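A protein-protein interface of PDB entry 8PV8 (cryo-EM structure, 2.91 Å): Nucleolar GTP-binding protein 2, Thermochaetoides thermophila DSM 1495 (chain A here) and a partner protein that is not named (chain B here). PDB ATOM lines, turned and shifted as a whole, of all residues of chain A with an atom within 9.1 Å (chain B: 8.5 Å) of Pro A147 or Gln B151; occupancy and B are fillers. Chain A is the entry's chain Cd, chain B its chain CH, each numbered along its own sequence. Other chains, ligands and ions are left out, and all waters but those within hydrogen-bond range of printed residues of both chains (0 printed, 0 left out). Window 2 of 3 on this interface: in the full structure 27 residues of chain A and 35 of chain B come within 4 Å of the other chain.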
ATOM      1  N   PHE A 141       8.985   9.304  29.276  1.00  0.00           N
ATOM      2  CA  PHE A 141       9.571  10.162  28.252  1.00  0.00           C
ATOM      3  C   PHE A 141      10.467  11.229  28.868  1.00  0.00           C
ATOM      4  O   PHE A 141      11.433  11.677  28.242  1.00  0.00           O
ATOM      5  CB  PHE A 141       8.469  10.812  27.417  1.00  0.00           C
ATOM      6  CG  PHE A 141       7.831   9.888  26.420  1.00  0.00           C
ATOM      7  CD1 PHE A 141       8.517   9.493  25.285  1.00  0.00           C
ATOM      8  CD2 PHE A 141       6.539   9.428  26.612  1.00  0.00           C
ATOM      9  CE1 PHE A 141       7.931   8.648  24.363  1.00  0.00           C
ATOM     10  CE2 PHE A 141       5.947   8.583  25.693  1.00  0.00           C
ATOM     11  CZ  PHE A 141       6.643   8.196  24.567  1.00  0.00           C
ATOM     12  N   SER A 142      10.153  11.657  30.094  1.00  0.00           N
ATOM     13  CA  SER A 142      10.965  12.670  30.759  1.00  0.00           C
ATOM     14  C   SER A 142      12.316  12.108  31.181  1.00  0.00           C
ATOM     15  O   SER A 142      13.320  12.828  31.194  1.00  0.00           O
ATOM     16  CB  SER A 142      10.221  13.226  31.971  1.00  0.00           C
ATOM     17  OG  SER A 142      10.161  12.265  33.009  1.00  0.00           O
ATOM     18  N   GLU A 143      12.361  10.821  31.534  1.00  0.00           N
ATOM     19  CA  GLU A 143      13.618  10.211  31.952  1.00  0.00           C
ATOM     20  C   GLU A 143      14.468   9.753  30.774  1.00  0.00           C
ATOM     21  O   GLU A 143      15.613   9.339  30.981  1.00  0.00           O
ATOM     22  CB  GLU A 143      13.345   9.028  32.881  1.00  0.00           C
ATOM     23  CG  GLU A 143      12.634   9.397  34.172  1.00  0.00           C
ATOM     24  CD  GLU A 143      12.563   8.231  35.136  1.00  0.00           C
ATOM     25  OE1 GLU A 143      13.182   7.187  34.842  1.00  0.00           O
ATOM     26  OE2 GLU A 143      11.891   8.357  36.182  1.00  0.00           O
ATOM     27  N   THR A 144      13.943   9.819  29.551  1.00  0.00           N
ATOM     28  CA  THR A 144      14.702   9.381  28.384  1.00  0.00           C
ATOM     29  C   THR A 144      15.523  10.524  27.793  1.00  0.00           C
ATOM     30  O   THR A 144      16.751  10.431  27.693  1.00  0.00           O
ATOM     31  CB  THR A 144      13.758   8.797  27.333  1.00  0.00           C
ATOM     32  OG1 THR A 144      12.980   7.744  27.919  1.00  0.00           O
ATOM     33  CG2 THR A 144      14.554   8.263  26.153  1.00  0.00           C
ATOM     34  N   PHE A 145      14.863  11.614  27.406  1.00  0.00           N
ATOM     35  CA  PHE A 145      15.536  12.774  26.838  1.00  0.00           C
ATOM     36  C   PHE A 145      14.916  14.064  27.360  1.00  0.00           C
ATOM     37  O   PHE A 145      13.695  14.161  27.508  1.00  0.00           O
ATOM     38  CB  PHE A 145      15.485  12.740  25.307  1.00  0.00           C
ATOM     39  CG  PHE A 145      16.212  13.875  24.658  1.00  0.00           C
ATOM     40  CD1 PHE A 145      17.594  13.886  24.604  1.00  0.00           C
ATOM     41  CD2 PHE A 145      15.511  14.928  24.093  1.00  0.00           C
ATOM     42  CE1 PHE A 145      18.269  14.934  24.005  1.00  0.00           C
ATOM     43  CE2 PHE A 145      16.179  15.984  23.502  1.00  0.00           C
ATOM     44  CZ  PHE A 145      17.556  15.987  23.454  1.00  0.00           C
ATOM     45  N   GLY A 146      15.769  15.053  27.650  1.00  0.00           N
ATOM     46  CA  GLY A 146      15.310  16.361  28.058  1.00  0.00           C
ATOM     47  C   GLY A 146      16.098  16.999  29.186  1.00  0.00           C
ATOM     48  O   GLY A 146      17.185  16.542  29.555  1.00  0.00           O
ATOM     49  N   PRO A 147      15.569  18.096  29.741  1.00  0.00           N
ATOM     50  CA  PRO A 147      16.250  18.723  30.887  1.00  0.00           C
ATOM     51  C   PRO A 147      16.218  17.865  32.137  1.00  0.00           C
ATOM     52  O   PRO A 147      17.131  17.957  32.965  1.00  0.00           O
ATOM     53  CB  PRO A 147      15.479  20.039  31.077  1.00  0.00           C
ATOM     54  CG  PRO A 147      14.156  19.790  30.466  1.00  0.00           C
ATOM     55  CD  PRO A 147      14.396  18.873  29.308  1.00  0.00           C
ATOM     56  N   LYS A 148      15.196  17.024  32.295  1.00  0.00           N
ATOM     57  CA  LYS A 148      15.068  16.156  33.458  1.00  0.00           C
ATOM     58  C   LYS A 148      15.565  14.744  33.165  1.00  0.00           C
ATOM     59  O   LYS A 148      15.297  13.822  33.942  1.00  0.00           O
ATOM     60  CB  LYS A 148      13.616  16.110  33.933  1.00  0.00           C
ATOM     61  CG  LYS A 148      12.944  17.463  34.217  1.00  0.00           C
ATOM     62  CD  LYS A 148      13.463  18.210  35.446  1.00  0.00           C
ATOM     63  CE  LYS A 148      14.451  19.318  35.082  1.00  0.00           C
ATOM     64  NZ  LYS A 148      14.842  20.130  36.265  1.00  0.00           N
ATOM     65  N   ALA A 149      16.267  14.559  32.048  1.00  0.00           N
ATOM     66  CA  ALA A 149      16.649  13.228  31.597  1.00  0.00           C
ATOM     67  C   ALA A 149      17.704  12.614  32.507  1.00  0.00           C
ATOM     68  O   ALA A 149      18.651  13.276  32.940  1.00  0.00           O
ATOM     69  CB  ALA A 149      17.174  13.282  30.165  1.00  0.00           C
ATOM     70  N   GLN A 150      17.524  11.326  32.796  1.00  0.00           N
ATOM     71  CA  GLN A 150      18.480  10.557  33.575  1.00  0.00           C
ATOM     72  C   GLN A 150      19.013   9.349  32.819  1.00  0.00           C
ATOM     73  O   GLN A 150      19.774   8.563  33.395  1.00  0.00           O
ATOM     74  CB  GLN A 150      17.848  10.101  34.897  1.00  0.00           C
ATOM     75  CG  GLN A 150      17.146  11.218  35.646  1.00  0.00           C
ATOM     76  CD  GLN A 150      18.107  12.273  36.147  1.00  0.00           C
ATOM     77  OE1 GLN A 150      19.265  11.986  36.447  1.00  0.00           O
ATOM     78  NE2 GLN A 150      17.636  13.512  36.219  1.00  0.00           N
ATOM     79  N   ARG A 151      18.633   9.178  31.554  1.00  0.00           N
ATOM     80  CA  ARG A 151      19.111   8.052  30.765  1.00  0.00           C
ATOM     81  C   ARG A 151      20.582   8.237  30.416  1.00  0.00           C
ATOM     82  O   ARG A 151      20.985   9.291  29.916  1.00  0.00           O
ATOM     83  CB  ARG A 151      18.277   7.911  29.493  1.00  0.00           C
ATOM     84  CG  ARG A 151      18.937   7.097  28.392  1.00  0.00           C
ATOM     85  CD  ARG A 151      18.018   6.952  27.198  1.00  0.00           C
ATOM     86  NE  ARG A 151      18.671   6.270  26.088  1.00  0.00           N
ATOM     87  CZ  ARG A 151      19.237   6.888  25.061  1.00  0.00           C
ATOM     88  NH1 ARG A 151      19.252   8.206  24.971  1.00  0.00           N
ATOM     89  NH2 ARG A 151      19.804   6.164  24.101  1.00  0.00           N
ATOM     90  N   VAL B  10       6.216  21.509  17.582  1.00  0.00           N
ATOM     91  CA  VAL B  10       5.261  20.575  18.170  1.00  0.00           C
ATOM     92  C   VAL B  10       4.772  21.169  19.485  1.00  0.00           C
ATOM     93  O   VAL B  10       5.547  21.224  20.451  1.00  0.00           O
ATOM     94  CB  VAL B  10       5.893  19.192  18.393  1.00  0.00           C
ATOM     95  CG1 VAL B  10       4.890  18.249  19.029  1.00  0.00           C
ATOM     96  CG2 VAL B  10       6.404  18.625  17.080  1.00  0.00           C
ATOM     97  N   PHE B  67       8.922  14.322  10.766  1.00  0.00           N
ATOM     98  CA  PHE B  67       9.932  13.647  11.563  1.00  0.00           C
ATOM     99  C   PHE B  67      10.596  12.550  10.735  1.00  0.00           C
ATOM    100  O   PHE B  67       9.936  11.915   9.905  1.00  0.00           O
ATOM    101  CB  PHE B  67       9.311  13.051  12.826  1.00  0.00           C
ATOM    102  CG  PHE B  67       9.330  13.978  14.005  1.00  0.00           C
ATOM    103  CD1 PHE B  67       8.326  14.914  14.182  1.00  0.00           C
ATOM    104  CD2 PHE B  67      10.351  13.917  14.934  1.00  0.00           C
ATOM    105  CE1 PHE B  67       8.338  15.767  15.262  1.00  0.00           C
ATOM    106  CE2 PHE B  67      10.365  14.771  16.014  1.00  0.00           C
ATOM    107  CZ  PHE B  67       9.360  15.695  16.178  1.00  0.00           C
ATOM    108  N   TYR B  85      18.634   8.921  21.274  1.00  0.00           N
ATOM    109  CA  TYR B  85      17.233   8.756  21.630  1.00  0.00           C
ATOM    110  C   TYR B  85      16.947   7.271  21.715  1.00  0.00           C
ATOM    111  O   TYR B  85      17.423   6.509  20.871  1.00  0.00           O
ATOM    112  CB  TYR B  85      16.350   9.367  20.548  1.00  0.00           C
ATOM    113  CG  TYR B  85      16.410  10.858  20.437  1.00  0.00           C
ATOM    114  CD1 TYR B  85      16.947  11.641  21.447  1.00  0.00           C
ATOM    115  CD2 TYR B  85      16.030  11.476  19.269  1.00  0.00           C
ATOM    116  CE1 TYR B  85      17.016  12.993  21.320  1.00  0.00           C
ATOM    117  CE2 TYR B  85      16.127  12.804  19.133  1.00  0.00           C
ATOM    118  CZ  TYR B  85      16.605  13.564  20.150  1.00  0.00           C
ATOM    119  OH  TYR B  85      16.651  14.906  19.957  1.00  0.00           O
ATOM    120  N   PHE B  90      10.987   6.750  20.550  1.00  0.00           N
ATOM    121  CA  PHE B  90      10.689   7.561  19.371  1.00  0.00           C
ATOM    122  C   PHE B  90       9.552   6.956  18.551  1.00  0.00           C
ATOM    123  O   PHE B  90       8.583   7.652  18.194  1.00  0.00           O
ATOM    124  CB  PHE B  90      11.972   7.686  18.543  1.00  0.00           C
ATOM    125  CG  PHE B  90      11.882   8.631  17.383  1.00  0.00           C
ATOM    126  CD1 PHE B  90      11.647   8.158  16.104  1.00  0.00           C
ATOM    127  CD2 PHE B  90      12.064   9.991  17.566  1.00  0.00           C
ATOM    128  CE1 PHE B  90      11.585   9.024  15.030  1.00  0.00           C
ATOM    129  CE2 PHE B  90      11.997  10.861  16.494  1.00  0.00           C
ATOM    130  CZ  PHE B  90      11.757  10.377  15.226  1.00  0.00           C
ATOM    131  N   ASP B 144       2.900  13.695  27.489  1.00  0.00           N
ATOM    132  CA  ASP B 144       4.328  13.381  27.489  1.00  0.00           C
ATOM    133  C   ASP B 144       4.947  13.211  26.093  1.00  0.00           C
ATOM    134  O   ASP B 144       6.049  13.744  25.868  1.00  0.00           O
ATOM    135  CB  ASP B 144       4.581  12.134  28.346  1.00  0.00           C
ATOM    136  CG  ASP B 144       4.328  12.379  29.819  1.00  0.00           C
ATOM    137  OD1 ASP B 144       4.503  13.530  30.270  1.00  0.00           O
ATOM    138  OD2 ASP B 144       3.950  11.422  30.527  1.00  0.00           O
ATOM    139  N   PRO B 145       4.331  12.479  25.138  1.00  0.00           N
ATOM    140  CA  PRO B 145       4.966  12.375  23.811  1.00  0.00           C
ATOM    141  C   PRO B 145       5.101  13.694  23.075  1.00  0.00           C
ATOM    142  O   PRO B 145       6.043  13.847  22.295  1.00  0.00           O
ATOM    143  CB  PRO B 145       4.049  11.407  23.053  1.00  0.00           C
ATOM    144  CG  PRO B 145       3.398  10.625  24.086  1.00  0.00           C
ATOM    145  CD  PRO B 145       3.154  11.583  25.193  1.00  0.00           C
ATOM    146  N   LEU B 146       4.205  14.656  23.303  1.00  0.00           N
ATOM    147  CA  LEU B 146       4.320  15.936  22.609  1.00  0.00           C
ATOM    148  C   LEU B 146       5.532  16.731  23.093  1.00  0.00           C
ATOM    149  O   LEU B 146       6.267  17.306  22.279  1.00  0.00           O
ATOM    150  CB  LEU B 146       3.033  16.739  22.780  1.00  0.00           C
ATOM    151  CG  LEU B 146       1.851  16.216  21.958  1.00  0.00           C
ATOM    152  CD1 LEU B 146       0.631  17.100  22.133  1.00  0.00           C
ATOM    153  CD2 LEU B 146       2.224  16.096  20.494  1.00  0.00           C
ATOM    154  N   ILE B 147       5.761  16.761  24.411  1.00  0.00           N
ATOM    155  CA  ILE B 147       6.952  17.407  24.959  1.00  0.00           C
ATOM    156  C   ILE B 147       8.211  16.696  24.483  1.00  0.00           C
ATOM    157  O   ILE B 147       9.193  17.341  24.075  1.00  0.00           O
ATOM    158  CB  ILE B 147       6.877  17.452  26.497  1.00  0.00           C
ATOM    159  CG1 ILE B 147       5.578  18.110  26.956  1.00  0.00           C
ATOM    160  CG2 ILE B 147       8.067  18.190  27.080  1.00  0.00           C
ATOM    161  CD1 ILE B 147       5.334  17.998  28.446  1.00  0.00           C
ATOM    162  N   TYR B 148       8.189  15.357  24.506  1.00  0.00           N
ATOM    163  CA  TYR B 148       9.328  14.572  24.039  1.00  0.00           C
ATOM    164  C   TYR B 148       9.648  14.872  22.579  1.00  0.00           C
ATOM    165  O   TYR B 148      10.806  15.112  22.231  1.00  0.00           O
ATOM    166  CB  TYR B 148       9.039  13.085  24.237  1.00  0.00           C
ATOM    167  CG  TYR B 148      10.054  12.147  23.628  1.00  0.00           C
ATOM    168  CD1 TYR B 148      11.256  11.885  24.269  1.00  0.00           C
ATOM    169  CD2 TYR B 148       9.798  11.503  22.421  1.00  0.00           C
ATOM    170  CE1 TYR B 148      12.180  11.023  23.723  1.00  0.00           C
ATOM    171  CE2 TYR B 148      10.719  10.640  21.868  1.00  0.00           C
ATOM    172  CZ  TYR B 148      11.906  10.404  22.524  1.00  0.00           C
ATOM    173  OH  TYR B 148      12.826   9.544  21.978  1.00  0.00           O
ATOM    174  N   LEU B 149       8.623  14.916  21.723  1.00  0.00           N
ATOM    175  CA  LEU B 149       8.845  15.147  20.302  1.00  0.00           C
ATOM    176  C   LEU B 149       9.276  16.578  20.016  1.00  0.00           C
ATOM    177  O   LEU B 149      10.043  16.806  19.078  1.00  0.00           O
ATOM    178  CB  LEU B 149       7.584  14.797  19.513  1.00  0.00           C
ATOM    179  CG  LEU B 149       7.327  13.301  19.319  1.00  0.00           C
ATOM    180  CD1 LEU B 149       5.966  13.062  18.681  1.00  0.00           C
ATOM    181  CD2 LEU B 149       8.438  12.675  18.495  1.00  0.00           C
ATOM    182  N   ASP B 150       8.808  17.554  20.804  1.00  0.00           N
ATOM    183  CA  ASP B 150       9.302  18.921  20.632  1.00  0.00           C
ATOM    184  C   ASP B 150      10.786  19.024  20.982  1.00  0.00           C
ATOM    185  O   ASP B 150      11.556  19.696  20.277  1.00  0.00           O
ATOM    186  CB  ASP B 150       8.483  19.896  21.478  1.00  0.00           C
ATOM    187  CG  ASP B 150       8.772  21.349  21.135  1.00  0.00           C
ATOM    188  OD1 ASP B 150       8.381  21.787  20.034  1.00  0.00           O
ATOM    189  OD2 ASP B 150       9.410  22.047  21.951  1.00  0.00           O
ATOM    190  N   GLN B 151      11.207  18.350  22.057  1.00  0.00           N
ATOM    191  CA  GLN B 151      12.626  18.307  22.414  1.00  0.00           C
ATOM    192  C   GLN B 151      13.453  17.607  21.336  1.00  0.00           C
ATOM    193  O   GLN B 151      14.553  18.061  20.976  1.00  0.00           O
ATOM    194  CB  GLN B 151      12.760  17.607  23.759  1.00  0.00           C
ATOM    195  CG  GLN B 151      12.140  18.414  24.868  1.00  0.00           C
ATOM    196  CD  GLN B 151      12.221  17.738  26.205  1.00  0.00           C
ATOM    197  OE1 GLN B 151      12.688  16.609  26.315  1.00  0.00           O
ATOM    198  NE2 GLN B 151      11.759  18.427  27.239  1.00  0.00           N
ATOM    199  N   VAL B 152      12.921  16.498  20.808  1.00  0.00           N
ATOM    200  CA  VAL B 152      13.507  15.804  19.659  1.00  0.00           C
ATOM    201  C   VAL B 152      13.649  16.726  18.457  1.00  0.00           C
ATOM    202  O   VAL B 152      14.682  16.725  17.779  1.00  0.00           O
ATOM    203  CB  VAL B 152      12.666  14.559  19.317  1.00  0.00           C
ATOM    204  CG1 VAL B 152      13.136  13.908  18.034  1.00  0.00           C
ATOM    205  CG2 VAL B 152      12.807  13.532  20.437  1.00  0.00           C
ATOM    206  N   ARG B 153      12.620  17.521  18.172  1.00  0.00           N
ATOM    207  CA  ARG B 153      12.655  18.417  17.023  1.00  0.00           C
ATOM    208  C   ARG B 153      13.734  19.477  17.181  1.00  0.00           C
ATOM    209  O   ARG B 153      14.460  19.787  16.229  1.00  0.00           O
ATOM    210  CB  ARG B 153      11.292  19.075  16.846  1.00  0.00           C
ATOM    211  CG  ARG B 153      11.252  20.122  15.771  1.00  0.00           C
ATOM    212  CD  ARG B 153      10.073  21.053  15.960  1.00  0.00           C
ATOM    213  NE  ARG B 153      10.220  21.930  17.117  1.00  0.00           N
ATOM    214  CZ  ARG B 153      10.842  23.101  17.086  1.00  0.00           C
ATOM    215  NH1 ARG B 153      11.427  23.543  15.986  1.00  0.00           N
ATOM    216  NH2 ARG B 153      10.888  23.842  18.190  1.00  0.00           N
ATOM    217  N   GLN B 154      13.848  20.051  18.384  1.00  0.00           N
ATOM    218  CA  GLN B 154      14.863  21.080  18.601  1.00  0.00           C
ATOM    219  C   GLN B 154      16.271  20.512  18.455  1.00  0.00           C
ATOM    220  O   GLN B 154      17.131  21.118  17.793  1.00  0.00           O
ATOM    221  CB  GLN B 154      14.691  21.732  19.974  1.00  0.00           C
ATOM    222  CG  GLN B 154      13.378  22.470  20.150  1.00  0.00           C
ATOM    223  CD  GLN B 154      13.386  23.410  21.340  1.00  0.00           C
ATOM    224  OE1 GLN B 154      14.385  23.534  22.047  1.00  0.00           O
ATOM    225  NE2 GLN B 154      12.257  24.067  21.576  1.00  0.00           N
ATOM    226  N   HIS B 155      16.519  19.332  19.027  1.00  0.00           N
ATOM    227  CA  HIS B 155      17.860  18.764  18.921  1.00  0.00           C
ATOM    228  C   HIS B 155      18.175  18.297  17.501  1.00  0.00           C
ATOM    229  O   HIS B 155      19.323  18.395  17.052  1.00  0.00           O
ATOM    230  CB  HIS B 155      18.028  17.637  19.924  1.00  0.00           C
ATOM    231  CG  HIS B 155      19.452  17.354  20.279  1.00  0.00           C
ATOM    232  ND1 HIS B 155      20.205  16.406  19.619  1.00  0.00           N
ATOM    233  CD2 HIS B 155      20.263  17.894  21.216  1.00  0.00           C
ATOM    234  CE1 HIS B 155      21.419  16.373  20.138  1.00  0.00           C
ATOM    235  NE2 HIS B 155      21.480  17.267  21.108  1.00  0.00           N
ATOM    236  N   LEU B 156      17.171  17.789  16.774  1.00  0.00           N
ATOM    237  CA  LEU B 156      17.380  17.438  15.370  1.00  0.00           C
ATOM    238  C   LEU B 156      17.646  18.672  14.521  1.00  0.00           C
ATOM    239  O   LEU B 156      18.401  18.608  13.544  1.00  0.00           O
ATOM    240  CB  LEU B 156      16.174  16.684  14.809  1.00  0.00           C
ATOM    241  CG  LEU B 156      15.953  15.207  15.128  1.00  0.00           C
ATOM    242  CD1 LEU B 156      14.523  14.828  14.802  1.00  0.00           C
ATOM    243  CD2 LEU B 156      16.918  14.349  14.344  1.00  0.00           C
ATOM    244  N   ALA B 157      17.003  19.794  14.851  1.00  0.00           N
ATOM    245  CA  ALA B 157      17.281  21.036  14.142  1.00  0.00           C
ATOM    246  C   ALA B 157      18.705  21.506  14.392  1.00  0.00           C
ATOM    247  O   ALA B 157      19.348  22.045  13.484  1.00  0.00           O
ATOM    248  CB  ALA B 157      16.280  22.116  14.553  1.00  0.00           C
ATOM    249  N   ARG B 158      19.220  21.302  15.605  1.00  0.00           N
ATOM    250  CA  ARG B 158      20.584  21.705  15.926  1.00  0.00           C
ATOM    251  C   ARG B 158      21.623  20.628  15.607  1.00  0.00           C
ATOM    252  O   ARG B 158      22.817  20.847  15.839  1.00  0.00           O
ATOM    253  CB  ARG B 158      20.684  22.108  17.395  1.00  0.00           C
ATOM    254  CG  ARG B 158      19.680  23.157  17.816  1.00  0.00           C
ATOM    255  CD  ARG B 158      20.023  23.703  19.181  1.00  0.00           C
ATOM    256  NE  ARG B 158      20.249  22.658  20.171  1.00  0.00           N
ATOM    257  CZ  ARG B 158      19.310  22.155  20.960  1.00  0.00           C
ATOM    258  NH1 ARG B 158      18.057  22.573  20.895  1.00  0.00           N
ATOM    259  NH2 ARG B 158      19.637  21.215  21.841  1.00  0.00           N
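OE1 of Gln B151 sits close to O of Phe A145.
O of Glu A143 lies within hydrogen-bond range of N of Arg A151, at 3.1 Å.
The side-chain hydroxyl (OH) of Tyr B85 sits close to the backbone carbonyl oxygen (O) of Val B152 (3.5 Å).
Among the printed residues, pairs that only touch across the chains: Phe A141 with Asp B144 (3.8 Å), Phe A141 with Pro B145 (3.6 Å), Phe A141 with Tyr B148 (3.5 Å), Phe A145 with Tyr B85 (3.5 Å), Phe A145 with His B155 (3.9 Å), Gly A146 with Gln B151 (3.2 Å), Pro A147 with Gln B151 (3.4 Å) and Arg A151 with Tyr B85 (3.8 Å).
Printed residues of chain B within 4 Å of Phe A141: Asp B144, Pro B145 and Tyr B148.
Gly A146 touches just one residue of chain B: Gln B151.
Of chain B, only Gln B151 comes within 4 Å of Pro A147.
Of the printed residues of chain B, Arg A151 touches Tyr B85 (3.8 Å).
Of the printed residues of chain A, Tyr B85 touches Phe A145 and Arg A151.
Of chain A, only Phe A145 (2.9 Å), Gly A146 (3.2 Å) and Pro A147 (3.4 Å) come within 4 Å of Gln B151.
No residue of chain A comes within 4 Å of Val B152.
Of the printed residues of chain A, His B155 touches Phe A145 (3.9 Å).
Leu B156 touches none of the printed residues of chain A.
The nearest printed residue of chain A that does not touch Tyr B148 is Phe A145 (4.05 Å).
Of the 11 printed residues of chain A, 5 touch a printed residue of chain B.
Printed residues of chain A that touch a printed residue of chain B: Phe A141, Phe A145, Gly A146, Pro A147 and Arg A151.
Hydrophobic or aromatic side chains of chain A that line the printed part of chain B: Phe A141, Phe A145 and Pro A147.
Of the 19 printed residues of chain B, 6 touch a printed residue of chain A.
Hydrophobic or aromatic side chains of chain B within 4 Å of the printed part of chain A: Tyr B85, Pro B145, Tyr B148 and His B155.
Among the printed residues, 9 pairs touch across the chains.
Among the printed residues, no Asp or Glu carboxylate lies within 4 Å of a Lys or Arg side-chain nitrogen of the other chain.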
